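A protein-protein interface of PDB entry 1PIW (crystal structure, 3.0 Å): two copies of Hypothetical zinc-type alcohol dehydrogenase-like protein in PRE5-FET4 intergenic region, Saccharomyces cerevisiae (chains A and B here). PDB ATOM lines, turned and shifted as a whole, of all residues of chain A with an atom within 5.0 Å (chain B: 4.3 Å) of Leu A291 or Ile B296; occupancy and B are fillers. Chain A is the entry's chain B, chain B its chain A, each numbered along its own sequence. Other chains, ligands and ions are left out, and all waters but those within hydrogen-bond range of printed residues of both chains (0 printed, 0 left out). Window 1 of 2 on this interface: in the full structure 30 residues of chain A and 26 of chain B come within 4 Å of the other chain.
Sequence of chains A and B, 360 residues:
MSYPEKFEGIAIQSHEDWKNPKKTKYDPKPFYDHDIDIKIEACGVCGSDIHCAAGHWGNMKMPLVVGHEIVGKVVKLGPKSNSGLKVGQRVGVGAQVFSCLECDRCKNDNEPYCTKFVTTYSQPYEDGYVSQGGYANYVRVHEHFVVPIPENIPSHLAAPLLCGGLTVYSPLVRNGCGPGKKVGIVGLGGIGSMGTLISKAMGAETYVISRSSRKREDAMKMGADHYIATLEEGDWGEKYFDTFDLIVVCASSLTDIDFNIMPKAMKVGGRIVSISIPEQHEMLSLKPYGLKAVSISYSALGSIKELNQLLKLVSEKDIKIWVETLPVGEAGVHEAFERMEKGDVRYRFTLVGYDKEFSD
N of Leu B284 lies within hydrogen-bond range of O of Leu A286 (3.0 Å). N of Tyr B298 is in hydrogen-bond range of O of Leu A291 (3.1 Å). The backbone NH of Ala A293 lies within hydrogen-bond range of the backbone carbonyl oxygen of Tyr B298, at 3.0 Å. The backbone NH (N) of Ile A296 is in hydrogen-bond range of the backbone carbonyl oxygen (O) of Ile B296.
N of Ile B272 sits at hydrogen-bond distance from O of Ser B295 (2.6 Å). The backbone carbonyl oxygen of Ile B272 lies within hydrogen-bond range of the backbone NH of Ser B297, at 2.8 Å.
Tyr A289 touches Tyr B298 (CA to CD2, 3.6 Å). Leu A291 touches Ile B296. CD2 of Tyr B298 touches CA of Lys A292 (3.7 Å). O of Val A294 touches O of Ile B296 (3.9 Å). Val A294 touches Ser B297 (O to CB, 3.1 Å). CB of Ser A295 touches CB of Ser B295, at 3.8 Å. CA of Ser A295 touches CB of Ser B297 (3.5 Å). Leu B291 touches Ile A296 (CD1 to O, 3.8 Å). Ile A296 touches Val B294. O of Ile A296 touches CA of Ser B295, at 3.7 Å.
Leu A291 touches just these residues of chain B: Ile B296 and Tyr B298. Ile B296 touches just these residues of chain A: Leu A291 (3.9 Å), Val A294 (3.9 Å), Ser A295 (3.2 Å) and Ile A296 (3.0 Å). Printed residues of chain A within 4 Å of Leu B284: Leu A286 (3.0 Å). Of the printed residues of chain B, Ala A293 touches Tyr B298 (3.0 Å). Of the printed residues of chain B, Val A294 touches Ile B296 (3.9 Å) and Ser B297 (3.1 Å). Of the printed residues of chain A, Ser B295 touches Ser A295 (3.8 Å) and Ile A296 (3.7 Å). Pro A263 touches none of the printed residues of chain B.
Hydrophobic or aromatic side chains of chain B that line the printed part of chain A: Leu B284, Leu B291, Ile B296 and Tyr B298. Of the 12 printed residues of chain A, 8 touch a printed residue of chain B. Hydrophobic or aromatic side chains of chain A that line the printed part of chain B: Tyr A289, Leu A291 and Ile A296. Among the printed residues, no Asp or Glu carboxylate lies within 4 Å of a Lys or Arg side-chain nitrogen of the other chain.
Leu A291 touches Ile B296, and with the chains exchanged Ile A296 touches Leu B291. Val A294 touches Ile B296, and with the chains exchanged Ile A296 touches Val B294. Ser A295 touches its own counterpart, Ser B295. Ser A295 touches Ile B296, and with the chains exchanged Ile A296 touches Ser B295. Of the 15 pairs that touch across the chains among the printed residues, 8 have their exchanged pair printed and touching as well.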
ATOM      1  N   PHE A 259     -32.436 -25.271 -13.040  1.00  0.00           N
ATOM      2  CA  PHE A 259     -31.548 -25.860 -14.032  1.00  0.00           C
ATOM      3  C   PHE A 259     -31.080 -27.232 -13.626  1.00  0.00           C
ATOM      4  O   PHE A 259     -30.499 -27.963 -14.424  1.00  0.00           O
ATOM      5  CB  PHE A 259     -30.339 -24.969 -14.283  1.00  0.00           C
ATOM      6  CG  PHE A 259     -30.692 -23.641 -14.853  1.00  0.00           C
ATOM      7  CD1 PHE A 259     -30.882 -22.543 -14.021  1.00  0.00           C
ATOM      8  CD2 PHE A 259     -30.882 -23.495 -16.217  1.00  0.00           C
ATOM      9  CE1 PHE A 259     -31.257 -21.315 -14.538  1.00  0.00           C
ATOM     10  CE2 PHE A 259     -31.259 -22.272 -16.749  1.00  0.00           C
ATOM     11  CZ  PHE A 259     -31.447 -21.177 -15.908  1.00  0.00           C
ATOM     12  N   PRO A 263     -33.184 -28.415 -17.755  1.00  0.00           N
ATOM     13  CA  PRO A 263     -32.292 -28.791 -18.855  1.00  0.00           C
ATOM     14  C   PRO A 263     -32.431 -30.258 -19.226  1.00  0.00           C
ATOM     15  O   PRO A 263     -32.518 -30.617 -20.400  1.00  0.00           O
ATOM     16  CB  PRO A 263     -30.911 -28.472 -18.299  1.00  0.00           C
ATOM     17  CG  PRO A 263     -31.172 -27.325 -17.392  1.00  0.00           C
ATOM     18  CD  PRO A 263     -32.421 -27.771 -16.672  1.00  0.00           C
ATOM     19  N   LEU A 286     -24.728 -21.651 -12.212  1.00  0.00           N
ATOM     20  CA  LEU A 286     -25.039 -23.031 -12.582  1.00  0.00           C
ATOM     21  C   LEU A 286     -23.699 -23.727 -12.759  1.00  0.00           C
ATOM     22  O   LEU A 286     -22.672 -23.067 -12.926  1.00  0.00           O
ATOM     23  CB  LEU A 286     -25.819 -23.071 -13.895  1.00  0.00           C
ATOM     24  CG  LEU A 286     -27.042 -22.159 -13.894  1.00  0.00           C
ATOM     25  CD1 LEU A 286     -27.696 -22.152 -15.255  1.00  0.00           C
ATOM     26  CD2 LEU A 286     -28.004 -22.633 -12.829  1.00  0.00           C
ATOM     27  N   LYS A 287     -23.698 -25.053 -12.712  1.00  0.00           N
ATOM     28  CA  LYS A 287     -22.454 -25.791 -12.870  1.00  0.00           C
ATOM     29  C   LYS A 287     -21.836 -25.494 -14.243  1.00  0.00           C
ATOM     30  O   LYS A 287     -22.550 -25.234 -15.217  1.00  0.00           O
ATOM     31  CB  LYS A 287     -22.708 -27.293 -12.701  1.00  0.00           C
ATOM     32  CG  LYS A 287     -22.012 -27.916 -11.487  1.00  0.00           C
ATOM     33  CD  LYS A 287     -22.383 -27.243 -10.166  1.00  0.00           C
ATOM     34  CE  LYS A 287     -21.618 -27.853  -8.985  1.00  0.00           C
ATOM     35  NZ  LYS A 287     -21.749 -27.063  -7.716  1.00  0.00           N
ATOM     36  N   TYR A 289     -20.754 -27.340 -16.206  1.00  0.00           N
ATOM     37  CA  TYR A 289     -21.256 -28.389 -17.078  1.00  0.00           C
ATOM     38  C   TYR A 289     -22.775 -28.585 -16.955  1.00  0.00           C
ATOM     39  O   TYR A 289     -23.292 -29.640 -17.323  1.00  0.00           O
ATOM     40  CB  TYR A 289     -20.527 -29.688 -16.727  1.00  0.00           C
ATOM     41  CG  TYR A 289     -20.637 -30.047 -15.253  1.00  0.00           C
ATOM     42  CD1 TYR A 289     -21.808 -30.612 -14.737  1.00  0.00           C
ATOM     43  CD2 TYR A 289     -19.587 -29.781 -14.365  1.00  0.00           C
ATOM     44  CE1 TYR A 289     -21.933 -30.903 -13.382  1.00  0.00           C
ATOM     45  CE2 TYR A 289     -19.703 -30.068 -13.000  1.00  0.00           C
ATOM     46  CZ  TYR A 289     -20.881 -30.629 -12.518  1.00  0.00           C
ATOM     47  OH  TYR A 289     -21.022 -30.914 -11.176  1.00  0.00           O
ATOM     48  N   GLY A 290     -23.485 -27.574 -16.452  1.00  0.00           N
ATOM     49  CA  GLY A 290     -24.928 -27.683 -16.283  1.00  0.00           C
ATOM     50  C   GLY A 290     -25.774 -27.626 -17.551  1.00  0.00           C
ATOM     51  O   GLY A 290     -26.676 -28.451 -17.752  1.00  0.00           O
ATOM     52  N   LEU A 291     -25.492 -26.640 -18.401  1.00  0.00           N
ATOM     53  CA  LEU A 291     -26.207 -26.458 -19.660  1.00  0.00           C
ATOM     54  C   LEU A 291     -25.534 -27.330 -20.718  1.00  0.00           C
ATOM     55  O   LEU A 291     -25.139 -26.846 -21.771  1.00  0.00           O
ATOM     56  CB  LEU A 291     -26.131 -24.991 -20.082  1.00  0.00           C
ATOM     57  CG  LEU A 291     -26.416 -23.985 -18.968  1.00  0.00           C
ATOM     58  CD1 LEU A 291     -25.975 -22.595 -19.374  1.00  0.00           C
ATOM     59  CD2 LEU A 291     -27.889 -24.002 -18.655  1.00  0.00           C
ATOM     60  N   LYS A 292     -25.396 -28.618 -20.433  1.00  0.00           N
ATOM     61  CA  LYS A 292     -24.751 -29.521 -21.373  1.00  0.00           C
ATOM     62  C   LYS A 292     -25.595 -29.675 -22.627  1.00  0.00           C
ATOM     63  O   LYS A 292     -26.628 -30.338 -22.613  1.00  0.00           O
ATOM     64  CB  LYS A 292     -24.523 -30.889 -20.732  1.00  0.00           C
ATOM     65  CG  LYS A 292     -23.590 -31.769 -21.544  1.00  0.00           C
ATOM     66  CD  LYS A 292     -23.327 -33.137 -20.918  1.00  0.00           C
ATOM     67  CE  LYS A 292     -22.477 -33.059 -19.663  1.00  0.00           C
ATOM     68  NZ  LYS A 292     -21.830 -34.375 -19.434  1.00  0.00           N
ATOM     69  N   ALA A 293     -25.145 -29.042 -23.707  1.00  0.00           N
ATOM     70  CA  ALA A 293     -25.828 -29.089 -24.988  1.00  0.00           C
ATOM     71  C   ALA A 293     -27.147 -28.333 -24.954  1.00  0.00           C
ATOM     72  O   ALA A 293     -28.013 -28.543 -25.800  1.00  0.00           O
ATOM     73  CB  ALA A 293     -26.058 -30.518 -25.399  1.00  0.00           C
ATOM     74  N   VAL A 294     -27.292 -27.448 -23.973  1.00  0.00           N
ATOM     75  CA  VAL A 294     -28.491 -26.626 -23.844  1.00  0.00           C
ATOM     76  C   VAL A 294     -28.113 -25.150 -23.700  1.00  0.00           C
ATOM     77  O   VAL A 294     -27.270 -24.796 -22.872  1.00  0.00           O
ATOM     78  CB  VAL A 294     -29.311 -27.041 -22.618  1.00  0.00           C
ATOM     79  CG1 VAL A 294     -30.424 -26.038 -22.356  1.00  0.00           C
ATOM     80  CG2 VAL A 294     -29.883 -28.409 -22.844  1.00  0.00           C
ATOM     81  N   SER A 295     -28.721 -24.288 -24.508  1.00  0.00           N
ATOM     82  CA  SER A 295     -28.418 -22.864 -24.412  1.00  0.00           C
ATOM     83  C   SER A 295     -29.462 -22.236 -23.513  1.00  0.00           C
ATOM     84  O   SER A 295     -30.465 -22.867 -23.186  1.00  0.00           O
ATOM     85  CB  SER A 295     -28.476 -22.185 -25.778  1.00  0.00           C
ATOM     86  OG  SER A 295     -29.816 -22.046 -26.209  1.00  0.00           O
ATOM     87  N   ILE A 296     -29.237 -20.994 -23.117  1.00  0.00           N
ATOM     88  CA  ILE A 296     -30.188 -20.331 -22.260  1.00  0.00           C
ATOM     89  C   ILE A 296     -30.027 -18.839 -22.495  1.00  0.00           C
ATOM     90  O   ILE A 296     -28.905 -18.324 -22.511  1.00  0.00           O
ATOM     91  CB  ILE A 296     -29.925 -20.717 -20.787  1.00  0.00           C
ATOM     92  CG1 ILE A 296     -31.198 -20.537 -19.962  1.00  0.00           C
ATOM     93  CG2 ILE A 296     -28.790 -19.899 -20.215  1.00  0.00           C
ATOM     94  CD1 ILE A 296     -31.693 -19.117 -19.882  1.00  0.00           C
ATOM     95  N   ILE B 272     -22.628 -17.891 -27.065  1.00  0.00           N
ATOM     96  CA  ILE B 272     -21.451 -18.117 -26.259  1.00  0.00           C
ATOM     97  C   ILE B 272     -21.473 -19.578 -25.833  1.00  0.00           C
ATOM     98  O   ILE B 272     -22.421 -20.044 -25.206  1.00  0.00           O
ATOM     99  CB  ILE B 272     -21.455 -17.192 -25.021  1.00  0.00           C
ATOM    100  CG1 ILE B 272     -21.580 -15.736 -25.489  1.00  0.00           C
ATOM    101  CG2 ILE B 272     -20.185 -17.380 -24.214  1.00  0.00           C
ATOM    102  CD1 ILE B 272     -21.407 -14.693 -24.406  1.00  0.00           C
ATOM    103  N   LEU B 284     -20.373 -21.212 -13.117  1.00  0.00           N
ATOM    104  CA  LEU B 284     -20.407 -20.334 -14.273  1.00  0.00           C
ATOM    105  C   LEU B 284     -21.365 -19.223 -13.819  1.00  0.00           C
ATOM    106  O   LEU B 284     -22.587 -19.408 -13.805  1.00  0.00           O
ATOM    107  CB  LEU B 284     -20.946 -21.089 -15.497  1.00  0.00           C
ATOM    108  CG  LEU B 284     -20.992 -20.317 -16.817  1.00  0.00           C
ATOM    109  CD1 LEU B 284     -19.689 -19.578 -17.018  1.00  0.00           C
ATOM    110  CD2 LEU B 284     -21.257 -21.271 -17.967  1.00  0.00           C
ATOM    111  N   LEU B 286     -22.972 -15.180 -13.816  1.00  0.00           N
ATOM    112  CA  LEU B 286     -23.288 -13.995 -14.601  1.00  0.00           C
ATOM    113  C   LEU B 286     -24.680 -13.459 -14.282  1.00  0.00           C
ATOM    114  O   LEU B 286     -25.576 -14.214 -13.894  1.00  0.00           O
ATOM    115  CB  LEU B 286     -23.185 -14.310 -16.099  1.00  0.00           C
ATOM    116  CG  LEU B 286     -23.947 -15.517 -16.666  1.00  0.00           C
ATOM    117  CD1 LEU B 286     -25.456 -15.292 -16.615  1.00  0.00           C
ATOM    118  CD2 LEU B 286     -23.502 -15.740 -18.102  1.00  0.00           C
ATOM    119  N   LEU B 291     -27.928 -11.823 -21.054  1.00  0.00           N
ATOM    120  CA  LEU B 291     -28.170 -12.831 -22.075  1.00  0.00           C
ATOM    121  C   LEU B 291     -29.328 -12.388 -22.966  1.00  0.00           C
ATOM    122  O   LEU B 291     -30.142 -13.205 -23.403  1.00  0.00           O
ATOM    123  CB  LEU B 291     -28.493 -14.168 -21.417  1.00  0.00           C
ATOM    124  CG  LEU B 291     -27.387 -14.732 -20.527  1.00  0.00           C
ATOM    125  CD1 LEU B 291     -27.940 -15.881 -19.734  1.00  0.00           C
ATOM    126  CD2 LEU B 291     -26.207 -15.173 -21.364  1.00  0.00           C
ATOM    127  N   VAL B 294     -28.667 -13.146 -26.648  1.00  0.00           N
ATOM    128  CA  VAL B 294     -27.408 -13.890 -26.677  1.00  0.00           C
ATOM    129  C   VAL B 294     -27.631 -15.187 -25.919  1.00  0.00           C
ATOM    130  O   VAL B 294     -28.233 -15.185 -24.851  1.00  0.00           O
ATOM    131  CB  VAL B 294     -26.261 -13.111 -25.996  1.00  0.00           C
ATOM    132  CG1 VAL B 294     -25.145 -14.050 -25.604  1.00  0.00           C
ATOM    133  CG2 VAL B 294     -25.713 -12.089 -26.942  1.00  0.00           C
ATOM    134  N   SER B 295     -27.151 -16.296 -26.463  1.00  0.00           N
ATOM    135  CA  SER B 295     -27.335 -17.572 -25.794  1.00  0.00           C
ATOM    136  C   SER B 295     -26.028 -18.129 -25.271  1.00  0.00           C
ATOM    137  O   SER B 295     -25.025 -18.162 -25.990  1.00  0.00           O
ATOM    138  CB  SER B 295     -27.966 -18.589 -26.752  1.00  0.00           C
ATOM    139  OG  SER B 295     -27.143 -18.835 -27.883  1.00  0.00           O
ATOM    140  N   ILE B 296     -26.034 -18.565 -24.016  1.00  0.00           N
ATOM    141  CA  ILE B 296     -24.840 -19.158 -23.428  1.00  0.00           C
ATOM    142  C   ILE B 296     -25.108 -20.648 -23.247  1.00  0.00           C
ATOM    143  O   ILE B 296     -26.221 -21.043 -22.905  1.00  0.00           O
ATOM    144  CB  ILE B 296     -24.512 -18.546 -22.056  1.00  0.00           C
ATOM    145  CG1 ILE B 296     -23.164 -19.071 -21.570  1.00  0.00           C
ATOM    146  CG2 ILE B 296     -25.582 -18.917 -21.050  1.00  0.00           C
ATOM    147  CD1 ILE B 296     -22.769 -18.566 -20.209  1.00  0.00           C
ATOM    148  N   SER B 297     -24.097 -21.474 -23.498  1.00  0.00           N
ATOM    149  CA  SER B 297     -24.246 -22.915 -23.344  1.00  0.00           C
ATOM    150  C   SER B 297     -22.898 -23.603 -23.205  1.00  0.00           C
ATOM    151  O   SER B 297     -21.878 -23.086 -23.648  1.00  0.00           O
ATOM    152  CB  SER B 297     -24.974 -23.512 -24.541  1.00  0.00           C
ATOM    153  OG  SER B 297     -24.055 -23.810 -25.574  1.00  0.00           O
ATOM    154  N   TYR B 298     -22.927 -24.781 -22.590  1.00  0.00           N
ATOM    155  CA  TYR B 298     -21.759 -25.615 -22.345  1.00  0.00           C
ATOM    156  C   TYR B 298     -21.673 -26.725 -23.399  1.00  0.00           C
ATOM    157  O   TYR B 298     -22.697 -27.231 -23.833  1.00  0.00           O
ATOM    158  CB  TYR B 298     -21.875 -26.249 -20.951  1.00  0.00           C
ATOM    159  CG  TYR B 298     -20.862 -27.351 -20.722  1.00  0.00           C
ATOM    160  CD1 TYR B 298     -19.508 -27.050 -20.605  1.00  0.00           C
ATOM    161  CD2 TYR B 298     -21.250 -28.704 -20.699  1.00  0.00           C
ATOM    162  CE1 TYR B 298     -18.557 -28.054 -20.479  1.00  0.00           C
ATOM    163  CE2 TYR B 298     -20.299 -29.724 -20.575  1.00  0.00           C
ATOM    164  CZ  TYR B 298     -18.945 -29.383 -20.468  1.00  0.00           C
ATOM    165  OH  TYR B 298     -17.957 -30.345 -20.375  1.00  0.00           O
